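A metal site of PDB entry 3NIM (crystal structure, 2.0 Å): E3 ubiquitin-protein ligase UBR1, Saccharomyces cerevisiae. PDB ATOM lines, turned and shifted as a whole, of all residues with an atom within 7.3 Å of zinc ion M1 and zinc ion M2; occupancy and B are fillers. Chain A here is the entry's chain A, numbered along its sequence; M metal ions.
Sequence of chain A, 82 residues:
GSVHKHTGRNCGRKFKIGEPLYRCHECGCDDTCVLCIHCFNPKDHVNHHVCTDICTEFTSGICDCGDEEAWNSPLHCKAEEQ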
ATOM      1  N   HIS A   4      -3.016  17.042  30.590  1.00  0.00           N
ATOM      2  CA  HIS A   4      -1.941  17.245  31.544  1.00  0.00           C
ATOM      3  C   HIS A   4      -1.512  18.667  31.284  1.00  0.00           C
ATOM      4  O   HIS A   4      -0.918  18.976  30.259  1.00  0.00           O
ATOM      5  CB  HIS A   4      -0.766  16.280  31.311  1.00  0.00           C
ATOM      6  CG  HIS A   4      -1.157  14.957  30.704  1.00  0.00           C
ATOM      7  ND1 HIS A   4      -0.928  14.642  29.374  1.00  0.00           N
ATOM      8  CD2 HIS A   4      -1.734  13.859  31.253  1.00  0.00           C
ATOM      9  CE1 HIS A   4      -1.352  13.417  29.130  1.00  0.00           C
ATOM     10  NE2 HIS A   4      -1.851  12.918  30.251  1.00  0.00           N
ATOM     11  N   LYS A   5      -1.880  19.554  32.203  1.00  0.00           N
ATOM     12  CA  LYS A   5      -1.629  20.975  32.063  1.00  0.00           C
ATOM     13  C   LYS A   5      -0.165  21.239  32.401  1.00  0.00           C
ATOM     14  O   LYS A   5       0.470  20.438  33.078  1.00  0.00           O
ATOM     15  CB  LYS A   5      -2.533  21.786  33.013  1.00  0.00           C
ATOM     16  CG  LYS A   5      -4.045  21.490  32.902  1.00  0.00           C
ATOM     17  CD  LYS A   5      -4.812  22.103  34.074  1.00  0.00           C
ATOM     18  CE  LYS A   5      -6.344  21.889  33.954  1.00  0.00           C
ATOM     19  NZ  LYS A   5      -6.732  20.448  34.024  1.00  0.00           N
ATOM     20  N   HIS A   6       0.358  22.361  31.911  1.00  0.00           N
ATOM     21  CA  HIS A   6       1.715  22.806  32.251  1.00  0.00           C
ATOM     22  C   HIS A   6       1.674  24.233  32.839  1.00  0.00           C
ATOM     23  O   HIS A   6       2.493  25.086  32.493  1.00  0.00           O
ATOM     24  CB  HIS A   6       2.609  22.740  31.002  1.00  0.00           C
ATOM     25  CG  HIS A   6       2.133  23.590  29.863  1.00  0.00           C
ATOM     26  ND1 HIS A   6       2.420  24.938  29.792  1.00  0.00           N
ATOM     27  CD2 HIS A   6       1.376  23.301  28.778  1.00  0.00           C
ATOM     28  CE1 HIS A   6       1.867  25.432  28.697  1.00  0.00           C
ATOM     29  NE2 HIS A   6       1.217  24.465  28.074  1.00  0.00           N
ATOM     30  N   ARG A   9       4.397  27.288  33.649  1.00  0.00           N
ATOM     31  CA  ARG A   9       5.604  26.975  32.870  1.00  0.00           C
ATOM     32  C   ARG A   9       5.301  26.695  31.388  1.00  0.00           C
ATOM     33  O   ARG A   9       4.149  26.609  31.000  1.00  0.00           O
ATOM     34  CB  ARG A   9       6.361  25.786  33.486  1.00  0.00           C
ATOM     35  CG  ARG A   9       5.489  24.581  33.786  1.00  0.00           C
ATOM     36  CD  ARG A   9       6.270  23.286  33.751  1.00  0.00           C
ATOM     37  NE  ARG A   9       6.655  22.943  32.389  1.00  0.00           N
ATOM     38  CZ  ARG A   9       7.352  21.869  32.054  1.00  0.00           C
ATOM     39  NH1 ARG A   9       7.780  21.024  32.972  1.00  0.00           N
ATOM     40  NH2 ARG A   9       7.628  21.646  30.782  1.00  0.00           N
ATOM     41  N   ASN A  10       6.348  26.515  30.600  1.00  0.00           N
ATOM     42  CA  ASN A  10       6.187  26.199  29.183  1.00  0.00           C
ATOM     43  C   ASN A  10       5.743  24.767  29.010  1.00  0.00           C
ATOM     44  O   ASN A  10       5.881  23.953  29.929  1.00  0.00           O
ATOM     45  CB  ASN A  10       7.494  26.404  28.427  1.00  0.00           C
ATOM     46  CG  ASN A  10       8.552  25.407  28.870  1.00  0.00           C
ATOM     47  OD1 ASN A  10       8.748  25.215  30.068  1.00  0.00           O
ATOM     48  ND2 ASN A  10       9.191  24.742  27.921  1.00  0.00           N
ATOM     49  N   CYS A  11       5.202  24.468  27.838  1.00  0.00           N
ATOM     50  CA  CYS A  11       4.910  23.104  27.449  1.00  0.00           C
ATOM     51  C   CYS A  11       6.182  22.279  27.248  1.00  0.00           C
ATOM     52  O   CYS A  11       6.443  21.343  28.007  1.00  0.00           O
ATOM     53  CB  CYS A  11       4.070  23.086  26.191  1.00  0.00           C
ATOM     54  SG  CYS A  11       3.638  21.396  25.711  1.00  0.00           S
ATOM     55  N   GLY A  12       6.941  22.605  26.203  1.00  0.00           N
ATOM     56  CA  GLY A  12       8.211  21.911  25.913  1.00  0.00           C
ATOM     57  C   GLY A  12       8.069  20.468  25.478  1.00  0.00           C
ATOM     58  O   GLY A  12       9.077  19.753  25.403  1.00  0.00           O
ATOM     59  N   ARG A  13       6.838  20.025  25.198  1.00  0.00           N
ATOM     60  CA  ARG A  13       6.562  18.623  24.814  1.00  0.00           C
ATOM     61  C   ARG A  13       7.174  18.303  23.455  1.00  0.00           C
ATOM     62  O   ARG A  13       7.025  19.062  22.516  1.00  0.00           O
ATOM     63  CB  ARG A  13       5.047  18.360  24.828  1.00  0.00           C
ATOM     64  CG  ARG A  13       4.590  17.004  24.274  1.00  0.00           C
ATOM     65  CD  ARG A  13       3.064  16.929  24.218  1.00  0.00           C
ATOM     66  NE  ARG A  13       2.558  15.612  23.826  1.00  0.00           N
ATOM     67  CZ  ARG A  13       2.512  15.144  22.575  1.00  0.00           C
ATOM     68  NH1 ARG A  13       2.958  15.874  21.539  1.00  0.00           N
ATOM     69  NH2 ARG A  13       2.004  13.935  22.350  1.00  0.00           N
ATOM     70  N   PHE A  15       7.249  16.584  19.989  1.00  0.00           N
ATOM     71  CA  PHE A  15       6.270  16.022  19.051  1.00  0.00           C
ATOM     72  C   PHE A  15       6.543  14.548  18.826  1.00  0.00           C
ATOM     73  O   PHE A  15       7.691  14.122  18.795  1.00  0.00           O
ATOM     74  CB  PHE A  15       6.290  16.787  17.712  1.00  0.00           C
ATOM     75  CG  PHE A  15       5.922  18.232  17.858  1.00  0.00           C
ATOM     76  CD1 PHE A  15       4.594  18.631  17.884  1.00  0.00           C
ATOM     77  CD2 PHE A  15       6.905  19.196  18.023  1.00  0.00           C
ATOM     78  CE1 PHE A  15       4.256  19.975  18.053  1.00  0.00           C
ATOM     79  CE2 PHE A  15       6.579  20.537  18.187  1.00  0.00           C
ATOM     80  CZ  PHE A  15       5.256  20.928  18.213  1.00  0.00           C
ATOM     81  N   VAL A  34       6.058  26.957  17.334  1.00  0.00           N
ATOM     82  CA  VAL A  34       5.078  25.885  17.088  1.00  0.00           C
ATOM     83  C   VAL A  34       4.298  25.448  18.364  1.00  0.00           C
ATOM     84  O   VAL A  34       4.780  25.645  19.490  1.00  0.00           O
ATOM     85  CB  VAL A  34       5.718  24.638  16.401  1.00  0.00           C
ATOM     86  CG1 VAL A  34       6.145  24.943  14.945  1.00  0.00           C
ATOM     87  CG2 VAL A  34       6.890  24.109  17.202  1.00  0.00           C
ATOM     88  N   LEU A  35       3.103  24.895  18.158  1.00  0.00           N
ATOM     89  CA  LEU A  35       2.273  24.387  19.270  1.00  0.00           C
ATOM     90  C   LEU A  35       1.848  22.956  19.000  1.00  0.00           C
ATOM     91  O   LEU A  35       1.715  22.538  17.843  1.00  0.00           O
ATOM     92  CB  LEU A  35       1.020  25.262  19.464  1.00  0.00           C
ATOM     93  CG  LEU A  35       1.190  26.748  19.827  1.00  0.00           C
ATOM     94  CD1 LEU A  35      -0.032  27.608  19.501  1.00  0.00           C
ATOM     95  CD2 LEU A  35       1.602  26.922  21.300  1.00  0.00           C
ATOM     96  N   CYS A  36       1.654  22.193  20.059  1.00  0.00           N
ATOM     97  CA  CYS A  36       1.260  20.795  19.918  1.00  0.00           C
ATOM     98  C   CYS A  36      -0.276  20.664  19.977  1.00  0.00           C
ATOM     99  O   CYS A  36      -0.998  21.624  20.262  1.00  0.00           O
ATOM    100  CB  CYS A  36       1.924  19.941  20.995  1.00  0.00           C
ATOM    101  SG  CYS A  36       1.218  20.222  22.625  1.00  0.00           S
ATOM    102  N   ILE A  37      -0.766  19.455  19.704  1.00  0.00           N
ATOM    103  CA  ILE A  37      -2.192  19.132  19.688  1.00  0.00           C
ATOM    104  C   ILE A  37      -2.858  19.416  21.058  1.00  0.00           C
ATOM    105  O   ILE A  37      -4.066  19.691  21.125  1.00  0.00           O
ATOM    106  CB  ILE A  37      -2.408  17.650  19.326  1.00  0.00           C
ATOM    107  CG1 ILE A  37      -1.443  16.761  20.139  1.00  0.00           C
ATOM    108  CG2 ILE A  37      -2.207  17.424  17.829  1.00  0.00           C
ATOM    109  CD1 ILE A  37      -1.689  15.270  20.095  1.00  0.00           C
ATOM    110  N   HIS A  38      -2.074  19.335  22.142  1.00  0.00           N
ATOM    111  CA  HIS A  38      -2.611  19.525  23.485  1.00  0.00           C
ATOM    112  C   HIS A  38      -2.891  21.006  23.724  1.00  0.00           C
ATOM    113  O   HIS A  38      -3.786  21.374  24.492  1.00  0.00           O
ATOM    114  CB  HIS A  38      -1.658  19.026  24.553  1.00  0.00           C
ATOM    115  CG  HIS A  38      -1.400  17.542  24.525  1.00  0.00           C
ATOM    116  ND1 HIS A  38      -1.683  16.754  23.436  1.00  0.00           N
ATOM    117  CD2 HIS A  38      -0.842  16.724  25.441  1.00  0.00           C
ATOM    118  CE1 HIS A  38      -1.327  15.507  23.686  1.00  0.00           C
ATOM    119  NE2 HIS A  38      -0.827  15.462  24.900  1.00  0.00           N
ATOM    120  N   CYS A  39      -2.112  21.855  23.057  1.00  0.00           N
ATOM    121  CA  CYS A  39      -2.000  23.266  23.449  1.00  0.00           C
ATOM    122  C   CYS A  39      -2.723  24.212  22.530  1.00  0.00           C
ATOM    123  O   CYS A  39      -3.292  25.217  22.990  1.00  0.00           O
ATOM    124  CB  CYS A  39      -0.517  23.651  23.528  1.00  0.00           C
ATOM    125  SG  CYS A  39       0.296  23.033  25.025  1.00  0.00           S
ATOM    126  N   PHE A  40      -2.649  23.924  21.232  1.00  0.00           N
ATOM    127  CA  PHE A  40      -3.230  24.762  20.186  1.00  0.00           C
ATOM    128  C   PHE A  40      -4.706  24.962  20.469  1.00  0.00           C
ATOM    129  O   PHE A  40      -5.456  23.999  20.534  1.00  0.00           O
ATOM    130  CB  PHE A  40      -3.038  24.092  18.826  1.00  0.00           C
ATOM    131  CG  PHE A  40      -3.615  24.873  17.690  1.00  0.00           C
ATOM    132  CD1 PHE A  40      -2.895  25.912  17.104  1.00  0.00           C
ATOM    133  CD2 PHE A  40      -4.892  24.567  17.208  1.00  0.00           C
ATOM    134  CE1 PHE A  40      -3.432  26.647  16.061  1.00  0.00           C
ATOM    135  CE2 PHE A  40      -5.453  25.298  16.169  1.00  0.00           C
ATOM    136  CZ  PHE A  40      -4.728  26.329  15.584  1.00  0.00           C
ATOM    137  N   ILE A  62      10.018  20.858  19.877  1.00  0.00           N
ATOM    138  CA  ILE A  62       9.201  20.880  21.110  1.00  0.00           C
ATOM    139  C   ILE A  62       8.187  22.004  21.021  1.00  0.00           C
ATOM    140  O   ILE A  62       8.406  22.978  20.292  1.00  0.00           O
ATOM    141  CB  ILE A  62      10.063  21.071  22.357  1.00  0.00           C
ATOM    142  CG1 ILE A  62      10.910  22.343  22.218  1.00  0.00           C
ATOM    143  CG2 ILE A  62      10.990  19.864  22.557  1.00  0.00           C
ATOM    144  CD1 ILE A  62      10.859  23.290  23.391  1.00  0.00           C
ATOM    145  N   CYS A  63       7.087  21.855  21.765  1.00  0.00           N
ATOM    146  CA  CYS A  63       6.007  22.825  21.754  1.00  0.00           C
ATOM    147  C   CYS A  63       6.380  24.111  22.498  1.00  0.00           C
ATOM    148  O   CYS A  63       6.891  24.049  23.626  1.00  0.00           O
ATOM    149  CB  CYS A  63       4.749  22.181  22.376  1.00  0.00           C
ATOM    150  SG  CYS A  63       3.440  23.345  22.645  1.00  0.00           S
ATOM    151  N   ASP A  64       6.105  25.280  21.887  1.00  0.00           N
ATOM    152  CA  ASP A  64       6.408  26.579  22.494  1.00  0.00           C
ATOM    153  C   ASP A  64       5.324  27.231  23.370  1.00  0.00           C
ATOM    154  O   ASP A  64       5.507  28.351  23.838  1.00  0.00           O
ATOM    155  CB  ASP A  64       6.879  27.581  21.443  1.00  0.00           C
ATOM    156  CG  ASP A  64       8.107  27.101  20.695  1.00  0.00           C
ATOM    157  OD1 ASP A  64       9.076  26.614  21.315  1.00  0.00           O
ATOM    158  OD2 ASP A  64       8.098  27.204  19.471  1.00  0.00           O
ATOM    159  N   CYS A  65       4.218  26.533  23.613  1.00  0.00           N
ATOM    160  CA  CYS A  65       3.186  27.075  24.479  1.00  0.00           C
ATOM    161  C   CYS A  65       3.736  27.440  25.865  1.00  0.00           C
ATOM    162  O   CYS A  65       4.410  26.641  26.469  1.00  0.00           O
ATOM    163  CB  CYS A  65       2.056  26.033  24.631  1.00  0.00           C
ATOM    164  SG  CYS A  65       0.602  26.710  25.396  1.00  0.00           S
ATOM    165  N   GLY A  66       3.448  28.649  26.344  1.00  0.00           N
ATOM    166  CA  GLY A  66       3.921  29.083  27.662  1.00  0.00           C
ATOM    167  C   GLY A  66       5.308  29.730  27.666  1.00  0.00           C
ATOM    168  O   GLY A  66       5.749  30.287  28.669  1.00  0.00           O
ATOM    169  N   LEU A  75      -1.511  33.506  24.626  1.00  0.00           N
ATOM    170  CA  LEU A  75      -2.213  32.273  24.230  1.00  0.00           C
ATOM    171  C   LEU A  75      -3.000  31.697  25.407  1.00  0.00           C
ATOM    172  O   LEU A  75      -2.612  31.830  26.565  1.00  0.00           O
ATOM    173  CB  LEU A  75      -1.254  31.196  23.715  1.00  0.00           C
ATOM    174  CG  LEU A  75      -0.348  31.429  22.508  1.00  0.00           C
ATOM    175  CD1 LEU A  75       0.491  30.198  22.265  1.00  0.00           C
ATOM    176  CD2 LEU A  75      -1.124  31.806  21.273  1.00  0.00           C
ATOM    177  N   HIS A  76      -4.095  31.032  25.074  1.00  0.00           N
ATOM    178  CA  HIS A  76      -4.942  30.415  26.082  1.00  0.00           C
ATOM    179  C   HIS A  76      -4.873  28.934  25.808  1.00  0.00           C
ATOM    180  O   HIS A  76      -5.667  28.390  25.061  1.00  0.00           O
ATOM    181  CB  HIS A  76      -6.354  30.974  25.969  1.00  0.00           C
ATOM    182  CG  HIS A  76      -6.394  32.475  25.969  1.00  0.00           C
ATOM    183  ND1 HIS A  76      -6.138  33.220  24.831  1.00  0.00           N
ATOM    184  CD2 HIS A  76      -6.603  33.362  26.966  1.00  0.00           C
ATOM    185  CE1 HIS A  76      -6.215  34.513  25.137  1.00  0.00           C
ATOM    186  NE2 HIS A  76      -6.490  34.616  26.421  1.00  0.00           N
ATOM    187  N   CYS A  77      -3.855  28.311  26.394  1.00  0.00           N
ATOM    188  CA  CYS A  77      -3.567  26.908  26.191  1.00  0.00           C
ATOM    189  C   CYS A  77      -4.853  26.123  26.246  1.00  0.00           C
ATOM    190  O   CYS A  77      -5.635  26.279  27.181  1.00  0.00           O
ATOM    191  CB  CYS A  77      -2.600  26.419  27.284  1.00  0.00           C
ATOM    192  SG  CYS A  77      -2.219  24.656  27.211  1.00  0.00           S
ATOM    193  N   LYS A  78      -5.057  25.256  25.253  1.00  0.00           N
ATOM    194  CA  LYS A  78      -6.216  24.352  25.206  1.00  0.00           C
ATOM    195  C   LYS A  78      -6.347  23.450  26.433  1.00  0.00           C
ATOM    196  O   LYS A  78      -7.464  23.182  26.878  1.00  0.00           O
ATOM    197  CB  LYS A  78      -6.192  23.496  23.937  1.00  0.00           C
ATOM    198  CG  LYS A  78      -7.542  22.837  23.643  1.00  0.00           C
ATOM    199  CD  LYS A  78      -7.481  21.872  22.483  1.00  0.00           C
ATOM    200  CE  LYS A  78      -8.858  21.280  22.228  1.00  0.00           C
ATOM    201  NZ  LYS A  78      -9.889  22.343  21.952  1.00  0.00           N
ATOM    202  N   ALA A  79      -5.226  22.982  26.967  1.00  0.00           N
ATOM    203  CA  ALA A  79      -5.233  22.093  28.139  1.00  0.00           C
ATOM    204  C   ALA A  79      -5.853  22.722  29.389  1.00  0.00           C
ATOM    205  O   ALA A  79      -6.344  22.023  30.279  1.00  0.00           O
ATOM    206  CB  ALA A  79      -3.803  21.618  28.442  1.00  0.00           C
ATOM    207  N   GLU A  80      -5.845  24.050  29.445  1.00  0.00           N
ATOM    208  CA  GLU A  80      -6.333  24.818  30.595  1.00  0.00           C
ATOM    209  C   GLU A  80      -7.855  24.964  30.631  1.00  0.00           C
ATOM    210  O   GLU A  80      -8.429  25.334  31.663  1.00  0.00           O
ATOM    211  CB  GLU A  80      -5.685  26.196  30.618  1.00  0.00           C
ATOM    212  CG  GLU A  80      -4.189  26.179  30.891  1.00  0.00           C
ATOM    213  CD  GLU A  80      -3.846  25.808  32.321  1.00  0.00           C
ATOM    214  OE1 GLU A  80      -4.627  26.158  33.238  1.00  0.00           O
ATOM    215  OE2 GLU A  80      -2.803  25.165  32.529  1.00  0.00           O
HETATM  216 ZN    ZN M   1       2.215  21.875  23.956  1.00  0.00          ZN
HETATM  217 ZN    ZN M   2      -0.022  24.695  26.436  1.00  0.00          ZN
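Of the 27 residues printed, 4 come within 4 Å of zinc ion M1.
Zinc ion M2 is bound by a ring nitrogen (NE2) of His 6, 2.1 Å away.
Zinc ion M2 is bound by the side-chain sulfur (SG) of Cys 39 (2.2 Å).
The side-chain sulfur (SG) of Cys 77 binds zinc ion M2 (2.3 Å).
Zinc ion M2 is bound by SG of Cys 65 (2.4 Å).
Zinc ion M1 is bound by SG of Cys 11 (2.3 Å), SG of Cys 63 (2.3 Å), SG of Cys 36 (2.3 Å) and SG of Cys 39 (2.5 Å).
Zinc ion M1 has four donor atoms within binding distance.
Within 4 Å of zinc ion M2: His 6, Cys 39, Cys 65 and Cys 77.
Along chain A the residues within 4 Å of zinc ion M2 span positions 6 to 77.
The nearest printed residue that does not touch zinc ion M2 is Cys 11 (4.4 Å).
The backbone carbonyl oxygen of Cys 11 sits at hydrogen-bond distance from the guanidinium group of Arg 9, 3.0 Å away.
N of Ala 79 lies close to SG of Cys 77 (3.5 Å).
The backbone carbonyl oxygen of Arg 9 is in hydrogen-bond range of a ring nitrogen (ND1) of His 6, 2.7 Å away.
The side-chain sulfur (SG) of Cys 63 lies close to the backbone NH (N) of Cys 65, 3.4 Å away.
The backbone carbonyl oxygen (O) of Cys 39 sits at hydrogen-bond distance from the backbone NH (N) of Lys 78 (2.9 Å).
The backbone NH (N) of Gly 12 sits at hydrogen-bond distance from the backbone carbonyl oxygen (O) of Cys 63, at 3.0 Å.
The backbone NH (N) of Cys 63 sits at hydrogen-bond distance from the backbone carbonyl oxygen (O) of Arg 13 (2.9 Å).
N of Cys 11 sits at hydrogen-bond distance from O of Cys 65 (2.7 Å).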
